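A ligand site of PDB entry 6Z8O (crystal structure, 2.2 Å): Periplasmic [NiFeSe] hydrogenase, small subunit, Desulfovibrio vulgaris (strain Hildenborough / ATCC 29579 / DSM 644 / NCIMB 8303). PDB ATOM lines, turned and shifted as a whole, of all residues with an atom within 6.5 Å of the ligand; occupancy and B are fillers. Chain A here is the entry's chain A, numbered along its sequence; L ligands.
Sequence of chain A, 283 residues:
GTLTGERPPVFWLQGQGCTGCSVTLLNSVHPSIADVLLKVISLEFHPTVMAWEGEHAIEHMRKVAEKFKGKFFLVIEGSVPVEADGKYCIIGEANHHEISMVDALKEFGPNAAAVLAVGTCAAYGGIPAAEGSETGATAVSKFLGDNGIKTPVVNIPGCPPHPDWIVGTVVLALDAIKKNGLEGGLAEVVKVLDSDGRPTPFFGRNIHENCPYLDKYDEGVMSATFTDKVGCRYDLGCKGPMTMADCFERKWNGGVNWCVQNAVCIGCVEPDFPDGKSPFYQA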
ATOM      1  N   ASN A 206      -8.984   8.798  10.062  1.00  0.00           N
ATOM      2  CA  ASN A 206      -9.940   7.706  10.051  1.00  0.00           C
ATOM      3  C   ASN A 206      -9.752   6.823   8.821  1.00  0.00           C
ATOM      4  O   ASN A 206      -9.316   7.282   7.764  1.00  0.00           O
ATOM      5  CB  ASN A 206     -11.370   8.280  10.087  1.00  0.00           C
ATOM      6  CG  ASN A 206     -12.421   7.268   9.721  1.00  0.00           C
ATOM      7  OD1 ASN A 206     -12.613   6.949   8.539  1.00  0.00           O
ATOM      8  ND2 ASN A 206     -13.120   6.746  10.720  1.00  0.00           N
ATOM      9  N   ILE A 207     -10.066   5.538   8.983  1.00  0.00           N
ATOM     10  CA  ILE A 207      -9.914   4.582   7.887  1.00  0.00           C
ATOM     11  C   ILE A 207     -10.917   4.902   6.778  1.00  0.00           C
ATOM     12  O   ILE A 207     -10.544   5.125   5.624  1.00  0.00           O
ATOM     13  CB  ILE A 207     -10.115   3.139   8.385  1.00  0.00           C
ATOM     14  CG1 ILE A 207      -9.132   2.790   9.516  1.00  0.00           C
ATOM     15  CG2 ILE A 207      -9.951   2.163   7.213  1.00  0.00           C
ATOM     16  CD1 ILE A 207      -7.731   2.470   9.064  1.00  0.00           C
ATOM     17  N   HIS A 208     -12.199   4.911   7.143  1.00  0.00           N
ATOM     18  CA  HIS A 208     -13.270   5.150   6.187  1.00  0.00           C
ATOM     19  C   HIS A 208     -12.992   6.410   5.359  1.00  0.00           C
ATOM     20  O   HIS A 208     -12.907   6.355   4.124  1.00  0.00           O
ATOM     21  CB  HIS A 208     -14.581   5.303   6.934  1.00  0.00           C
ATOM     22  CG  HIS A 208     -15.787   5.267   6.066  1.00  0.00           C
ATOM     23  ND1 HIS A 208     -16.337   4.089   5.595  1.00  0.00           N
ATOM     24  CD2 HIS A 208     -16.497   6.265   5.502  1.00  0.00           C
ATOM     25  CE1 HIS A 208     -17.376   4.362   4.835  1.00  0.00           C
ATOM     26  NE2 HIS A 208     -17.494   5.682   4.750  1.00  0.00           N
ATOM     27  N   GLU A 209     -12.859   7.543   6.046  1.00  0.00           N
ATOM     28  CA  GLU A 209     -12.692   8.831   5.373  1.00  0.00           C
ATOM     29  C   GLU A 209     -11.562   8.809   4.355  1.00  0.00           C
ATOM     30  O   GLU A 209     -11.529   9.675   3.473  1.00  0.00           O
ATOM     31  CB  GLU A 209     -12.422   9.914   6.423  1.00  0.00           C
ATOM     32  CG  GLU A 209     -13.602  10.188   7.341  1.00  0.00           C
ATOM     33  CD  GLU A 209     -13.240  11.145   8.459  1.00  0.00           C
ATOM     34  OE1 GLU A 209     -13.680  10.912   9.607  1.00  0.00           O
ATOM     35  OE2 GLU A 209     -12.509  12.124   8.198  1.00  0.00           O
ATOM     36  N   CYS A 211     -10.567   5.596   2.968  1.00  0.00           N
ATOM     37  CA  CYS A 211     -10.579   4.307   2.305  1.00  0.00           C
ATOM     38  C   CYS A 211     -10.645   4.500   0.799  1.00  0.00           C
ATOM     39  O   CYS A 211     -11.312   5.425   0.311  1.00  0.00           O
ATOM     40  CB  CYS A 211     -11.758   3.465   2.776  1.00  0.00           C
ATOM     41  SG  CYS A 211     -11.707   1.760   2.158  1.00  0.00           S
ATOM     42  N   PRO A 212      -9.950   3.665   0.017  1.00  0.00           N
ATOM     43  CA  PRO A 212     -10.089   3.754  -1.449  1.00  0.00           C
ATOM     44  C   PRO A 212     -11.377   3.157  -1.993  1.00  0.00           C
ATOM     45  O   PRO A 212     -11.693   3.392  -3.164  1.00  0.00           O
ATOM     46  CB  PRO A 212      -8.866   2.974  -1.956  1.00  0.00           C
ATOM     47  CG  PRO A 212      -8.506   2.055  -0.832  1.00  0.00           C
ATOM     48  CD  PRO A 212      -8.828   2.804   0.418  1.00  0.00           C
ATOM     49  N   TYR A 213     -12.126   2.410  -1.178  1.00  0.00           N
ATOM     50  CA  TYR A 213     -13.418   1.880  -1.594  1.00  0.00           C
ATOM     51  C   TYR A 213     -14.557   2.788  -1.154  1.00  0.00           C
ATOM     52  O   TYR A 213     -15.723   2.386  -1.247  1.00  0.00           O
ATOM     53  CB  TYR A 213     -13.612   0.470  -1.025  1.00  0.00           C
ATOM     54  CG  TYR A 213     -12.522  -0.513  -1.406  1.00  0.00           C
ATOM     55  CD1 TYR A 213     -12.332  -0.897  -2.731  1.00  0.00           C
ATOM     56  CD2 TYR A 213     -11.670  -1.035  -0.437  1.00  0.00           C
ATOM     57  CE1 TYR A 213     -11.332  -1.784  -3.075  1.00  0.00           C
ATOM     58  CE2 TYR A 213     -10.671  -1.923  -0.780  1.00  0.00           C
ATOM     59  CZ  TYR A 213     -10.502  -2.298  -2.099  1.00  0.00           C
ATOM     60  OH  TYR A 213      -9.506  -3.191  -2.430  1.00  0.00           O
ATOM     61  N   LEU A 214     -14.239   3.994  -0.686  1.00  0.00           N
ATOM     62  CA  LEU A 214     -15.270   4.913  -0.220  1.00  0.00           C
ATOM     63  C   LEU A 214     -16.262   5.230  -1.320  1.00  0.00           C
ATOM     64  O   LEU A 214     -17.454   5.415  -1.063  1.00  0.00           O
ATOM     65  CB  LEU A 214     -14.601   6.186   0.330  1.00  0.00           C
ATOM     66  CG  LEU A 214     -15.477   7.296   0.916  1.00  0.00           C
ATOM     67  CD1 LEU A 214     -16.398   6.775   1.997  1.00  0.00           C
ATOM     68  CD2 LEU A 214     -14.587   8.408   1.476  1.00  0.00           C
ATOM     69  N   ASP A 215     -15.777   5.322  -2.560  1.00  0.00           N
ATOM     70  CA  ASP A 215     -16.685   5.469  -3.698  1.00  0.00           C
ATOM     71  C   ASP A 215     -17.710   4.343  -3.734  1.00  0.00           C
ATOM     72  O   ASP A 215     -18.917   4.579  -3.854  1.00  0.00           O
ATOM     73  CB  ASP A 215     -15.891   5.533  -5.008  1.00  0.00           C
ATOM     74  CG  ASP A 215     -15.109   4.259  -5.269  1.00  0.00           C
ATOM     75  OD1 ASP A 215     -14.322   3.849  -4.381  1.00  0.00           O
ATOM     76  OD2 ASP A 215     -15.273   3.667  -6.358  1.00  0.00           O
ATOM     77  N   LYS A 216     -17.250   3.083  -3.612  1.00  0.00           N
ATOM     78  CA  LYS A 216     -18.184   1.960  -3.606  1.00  0.00           C
ATOM     79  C   LYS A 216     -19.156   2.067  -2.448  1.00  0.00           C
ATOM     80  O   LYS A 216     -20.331   1.697  -2.562  1.00  0.00           O
ATOM     81  CB  LYS A 216     -17.424   0.638  -3.546  1.00  0.00           C
ATOM     82  CG  LYS A 216     -16.332   0.498  -4.599  1.00  0.00           C
ATOM     83  CD  LYS A 216     -16.918   0.465  -5.999  1.00  0.00           C
ATOM     84  CE  LYS A 216     -15.847   0.549  -7.052  1.00  0.00           C
ATOM     85  NZ  LYS A 216     -16.457   0.887  -8.371  1.00  0.00           N
ATOM     86  N   TYR A 217     -18.688   2.574  -1.303  1.00  0.00           N
ATOM     87  CA  TYR A 217     -19.569   2.832  -0.177  1.00  0.00           C
ATOM     88  C   TYR A 217     -20.684   3.797  -0.589  1.00  0.00           C
ATOM     89  O   TYR A 217     -21.870   3.502  -0.424  1.00  0.00           O
ATOM     90  CB  TYR A 217     -18.762   3.391   0.993  1.00  0.00           C
ATOM     91  CG  TYR A 217     -19.573   3.766   2.218  1.00  0.00           C
ATOM     92  CD1 TYR A 217     -20.233   2.806   2.963  1.00  0.00           C
ATOM     93  CD2 TYR A 217     -19.649   5.088   2.642  1.00  0.00           C
ATOM     94  CE1 TYR A 217     -20.964   3.138   4.081  1.00  0.00           C
ATOM     95  CE2 TYR A 217     -20.380   5.436   3.767  1.00  0.00           C
ATOM     96  CZ  TYR A 217     -21.031   4.462   4.485  1.00  0.00           C
ATOM     97  OH  TYR A 217     -21.761   4.794   5.604  1.00  0.00           O
ATOM     98  N   MET A 222     -21.812  -3.171  -2.539  1.00  0.00           N
ATOM     99  CA  MET A 222     -21.165  -3.907  -1.467  1.00  0.00           C
ATOM    100  C   MET A 222     -20.774  -5.292  -1.981  1.00  0.00           C
ATOM    101  O   MET A 222     -21.366  -5.808  -2.926  1.00  0.00           O
ATOM    102  CB  MET A 222     -22.083  -4.033  -0.240  1.00  0.00           C
ATOM    103  CG  MET A 222     -22.668  -2.700   0.240  1.00  0.00           C
ATOM    104  SD  MET A 222     -21.471  -1.640   1.082  1.00  0.00           S
ATOM    105  CE  MET A 222     -22.368  -0.089   1.142  1.00  0.00           C
ATOM    106  N   GLY A 231     -16.253  -4.339  -4.440  1.00  0.00           N
ATOM    107  CA  GLY A 231     -17.146  -3.477  -3.700  1.00  0.00           C
ATOM    108  C   GLY A 231     -16.568  -3.009  -2.377  1.00  0.00           C
ATOM    109  O   GLY A 231     -15.444  -3.334  -1.993  1.00  0.00           O
ATOM    110  N   CYS A 232     -17.378  -2.239  -1.668  1.00  0.00           N
ATOM    111  CA  CYS A 232     -17.084  -1.870  -0.297  1.00  0.00           C
ATOM    112  C   CYS A 232     -17.409  -3.042   0.618  1.00  0.00           C
ATOM    113  O   CYS A 232     -18.273  -3.873   0.321  1.00  0.00           O
ATOM    114  CB  CYS A 232     -17.879  -0.626   0.098  1.00  0.00           C
ATOM    115  SG  CYS A 232     -18.083  -0.391   1.871  1.00  0.00           S
ATOM    116  N   ARG A 233     -16.705  -3.104   1.751  1.00  0.00           N
ATOM    117  CA  ARG A 233     -16.788  -4.256   2.644  1.00  0.00           C
ATOM    118  C   ARG A 233     -17.744  -4.062   3.819  1.00  0.00           C
ATOM    119  O   ARG A 233     -17.850  -4.963   4.659  1.00  0.00           O
ATOM    120  CB  ARG A 233     -15.388  -4.592   3.177  1.00  0.00           C
ATOM    121  CG  ARG A 233     -14.495  -5.366   2.190  1.00  0.00           C
ATOM    122  CD  ARG A 233     -14.047  -4.532   0.990  1.00  0.00           C
ATOM    123  NE  ARG A 233     -12.865  -5.121   0.361  1.00  0.00           N
ATOM    124  CZ  ARG A 233     -12.483  -4.887  -0.896  1.00  0.00           C
ATOM    125  NH1 ARG A 233     -13.197  -4.092  -1.686  1.00  0.00           N
ATOM    126  NH2 ARG A 233     -11.379  -5.461  -1.367  1.00  0.00           N
ATOM    127  N   TYR A 234     -18.428  -2.929   3.907  1.00  0.00           N
ATOM    128  CA  TYR A 234     -19.258  -2.643   5.074  1.00  0.00           C
ATOM    129  C   TYR A 234     -20.221  -3.787   5.410  1.00  0.00           C
ATOM    130  O   TYR A 234     -20.406  -4.126   6.584  1.00  0.00           O
ATOM    131  CB  TYR A 234     -20.048  -1.344   4.855  1.00  0.00           C
ATOM    132  CG  TYR A 234     -20.988  -1.015   5.987  1.00  0.00           C
ATOM    133  CD1 TYR A 234     -20.567  -0.335   7.118  1.00  0.00           C
ATOM    134  CD2 TYR A 234     -22.319  -1.400   5.918  1.00  0.00           C
ATOM    135  CE1 TYR A 234     -21.440  -0.051   8.147  1.00  0.00           C
ATOM    136  CE2 TYR A 234     -23.196  -1.115   6.931  1.00  0.00           C
ATOM    137  CZ  TYR A 234     -22.763  -0.441   8.047  1.00  0.00           C
ATOM    138  OH  TYR A 234     -23.656  -0.166   9.051  1.00  0.00           O
ATOM    139  N   ASP A 235     -20.836  -4.391   4.391  1.00  0.00           N
ATOM    140  CA  ASP A 235     -21.817  -5.439   4.675  1.00  0.00           C
ATOM    141  C   ASP A 235     -21.163  -6.701   5.211  1.00  0.00           C
ATOM    142  O   ASP A 235     -21.803  -7.461   5.956  1.00  0.00           O
ATOM    143  CB  ASP A 235     -22.621  -5.784   3.419  1.00  0.00           C
ATOM    144  CG  ASP A 235     -23.464  -4.632   2.929  1.00  0.00           C
ATOM    145  OD1 ASP A 235     -23.585  -3.620   3.655  1.00  0.00           O
ATOM    146  OD2 ASP A 235     -24.042  -4.759   1.823  1.00  0.00           O
ATOM    147  N   CYS A 238     -16.881  -4.581   7.824  1.00  0.00           N
ATOM    148  CA  CYS A 238     -15.780  -3.643   8.008  1.00  0.00           C
ATOM    149  C   CYS A 238     -16.151  -2.606   9.063  1.00  0.00           C
ATOM    150  O   CYS A 238     -17.291  -2.129   9.122  1.00  0.00           O
ATOM    151  CB  CYS A 238     -15.444  -2.942   6.685  1.00  0.00           C
ATOM    152  SG  CYS A 238     -14.101  -1.733   6.824  1.00  0.00           S
ATOM    153  N   LYS A 239     -15.181  -2.266   9.905  1.00  0.00           N
ATOM    154  CA  LYS A 239     -15.379  -1.293  10.972  1.00  0.00           C
ATOM    155  C   LYS A 239     -14.588  -0.016  10.715  1.00  0.00           C
ATOM    156  O   LYS A 239     -14.374   0.780  11.640  1.00  0.00           O
ATOM    157  CB  LYS A 239     -15.000  -1.892  12.326  1.00  0.00           C
ATOM    158  CG  LYS A 239     -15.727  -3.188  12.680  1.00  0.00           C
ATOM    159  CD  LYS A 239     -17.222  -3.114  12.392  1.00  0.00           C
ATOM    160  CE  LYS A 239     -17.981  -4.280  13.026  1.00  0.00           C
ATOM    161  NZ  LYS A 239     -17.381  -5.613  12.715  1.00  0.00           N
ATOM    162  N   GLY A 240     -14.151   0.203   9.466  1.00  0.00           N
ATOM    163  CA  GLY A 240     -13.499   1.437   9.107  1.00  0.00           C
ATOM    164  C   GLY A 240     -14.238   2.683   9.517  1.00  0.00           C
ATOM    165  O   GLY A 240     -13.596   3.670   9.912  1.00  0.00           O
ATOM    166  N   PRO A 241     -15.570   2.706   9.442  1.00  0.00           N
ATOM    167  CA  PRO A 241     -16.294   3.934   9.818  1.00  0.00           C
ATOM    168  C   PRO A 241     -15.958   4.472  11.206  1.00  0.00           C
ATOM    169  O   PRO A 241     -15.947   5.697  11.378  1.00  0.00           O
ATOM    170  CB  PRO A 241     -17.766   3.477   9.737  1.00  0.00           C
ATOM    171  CG  PRO A 241     -17.755   2.459   8.663  1.00  0.00           C
ATOM    172  CD  PRO A 241     -16.480   1.695   8.878  1.00  0.00           C
ATOM    173  N   TRP A 258      -3.325  -5.272   3.368  1.00  0.00           N
ATOM    174  CA  TRP A 258      -3.831  -4.797   4.653  1.00  0.00           C
ATOM    175  C   TRP A 258      -5.272  -5.255   4.809  1.00  0.00           C
ATOM    176  O   TRP A 258      -5.872  -5.856   3.905  1.00  0.00           O
ATOM    177  CB  TRP A 258      -3.695  -3.288   4.793  1.00  0.00           C
ATOM    178  CG  TRP A 258      -4.554  -2.542   3.873  1.00  0.00           C
ATOM    179  CD1 TRP A 258      -4.537  -2.594   2.518  1.00  0.00           C
ATOM    180  CD2 TRP A 258      -5.562  -1.611   4.232  1.00  0.00           C
ATOM    181  NE1 TRP A 258      -5.489  -1.745   2.001  1.00  0.00           N
ATOM    182  CE2 TRP A 258      -6.136  -1.124   3.039  1.00  0.00           C
ATOM    183  CE3 TRP A 258      -6.051  -1.126   5.447  1.00  0.00           C
ATOM    184  CZ2 TRP A 258      -7.167  -0.191   3.023  1.00  0.00           C
ATOM    185  CZ3 TRP A 258      -7.073  -0.197   5.439  1.00  0.00           C
ATOM    186  CH2 TRP A 258      -7.616   0.253   4.232  1.00  0.00           C
ATOM    187  N   VAL A 260      -8.490  -4.133   5.159  1.00  0.00           N
ATOM    188  CA  VAL A 260      -9.675  -3.865   4.342  1.00  0.00           C
ATOM    189  C   VAL A 260      -9.530  -4.533   2.991  1.00  0.00           C
ATOM    190  O   VAL A 260     -10.477  -5.147   2.477  1.00  0.00           O
ATOM    191  CB  VAL A 260      -9.904  -2.359   4.177  1.00  0.00           C
ATOM    192  CG1 VAL A 260     -10.937  -2.109   3.087  1.00  0.00           C
ATOM    193  CG2 VAL A 260     -10.340  -1.734   5.495  1.00  0.00           C
ATOM    194  N   CYS A 265     -11.889  -4.696   8.277  1.00  0.00           N
ATOM    195  CA  CYS A 265     -11.277  -4.012   9.406  1.00  0.00           C
ATOM    196  C   CYS A 265     -12.113  -4.302  10.644  1.00  0.00           C
ATOM    197  O   CYS A 265     -13.345  -4.241  10.603  1.00  0.00           O
ATOM    198  CB  CYS A 265     -11.198  -2.512   9.150  1.00  0.00           C
ATOM    199  SG  CYS A 265     -10.287  -1.575  10.392  1.00  0.00           S
HETATM  200 FE1  LIG L   1     -14.731  -0.418   5.041  1.00  0.00          FE
HETATM  201 FE2  LIG L   1     -15.524   2.180   4.981  1.00  0.00          FE
HETATM  202 FE3  LIG L   1     -16.266   0.463   2.994  1.00  0.00          FE
HETATM  203 FE4  LIG L   1     -13.698   1.260   3.179  1.00  0.00          FE
HETATM  204  S1  LIG L   1     -15.506   2.621   2.725  1.00  0.00           S
HETATM  205  S2  LIG L   1     -14.426  -0.888   2.806  1.00  0.00           S
HETATM  206  S3  LIG L   1     -13.402   1.420   5.457  1.00  0.00           S
HETATM  207  S4  LIG L   1     -16.893   0.344   5.208  1.00  0.00           S
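ND1 of His 208 is bound to FE2 of the ligand. SG of Cys 211 is bound to FE4 of the ligand, 2.3 Å away. An iron atom (FE3) of the ligand is bound by the side-chain sulfur (SG) of Cys 232 (2.3 Å). The side-chain sulfur (SG) of Cys 238 is bound to an iron atom (FE1) of the ligand (2.3 Å). The backbone NH (N) of Arg 233 lies close to a sulfur (S2) of the ligand (3.3 Å).
N of His 208 sits at hydrogen-bond distance from O of Gly 240 (3.3 Å). N of His 208 lies within hydrogen-bond range of OD1 of Asn 206, 2.5 Å away. The side-chain sulfur of Cys 211 lies close to the backbone NH of Tyr 213 (3.4 Å). N of Tyr 234 lies close to SG of Cys 232. The side-chain sulfur (SG) of Cys 238 sits close to the backbone NH (N) of Gly 240, 3.3 Å away. NE of Arg 233 lies within hydrogen-bond range of O of Val 260 (3.2 Å). The side-chain amide nitrogen (ND2) of Asn 206 sits at hydrogen-bond distance from the backbone carbonyl oxygen (O) of Gly 240. The backbone carbonyl oxygen of Pro 241 lies within hydrogen-bond range of the side-chain amide nitrogen of Asn 206, at 3.1 Å.
Ile 207 touches the ligand (CG2 to S3, 3.9 Å). O of Tyr 213 touches S1 of the ligand (3.98 Å). CA of Leu 214 touches S1 of the ligand (3.7 Å). Tyr 217 touches the ligand. Tyr 234 touches the ligand. CA of Gly 240 touches S3 of the ligand (3.7 Å). Pro 241 touches the ligand (CD to S4, 3.9 Å). Val 260 touches the ligand (CG1 to S2, 3.7 Å). Along chain A the residues within 4 Å of the ligand span positions 207 to 260.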
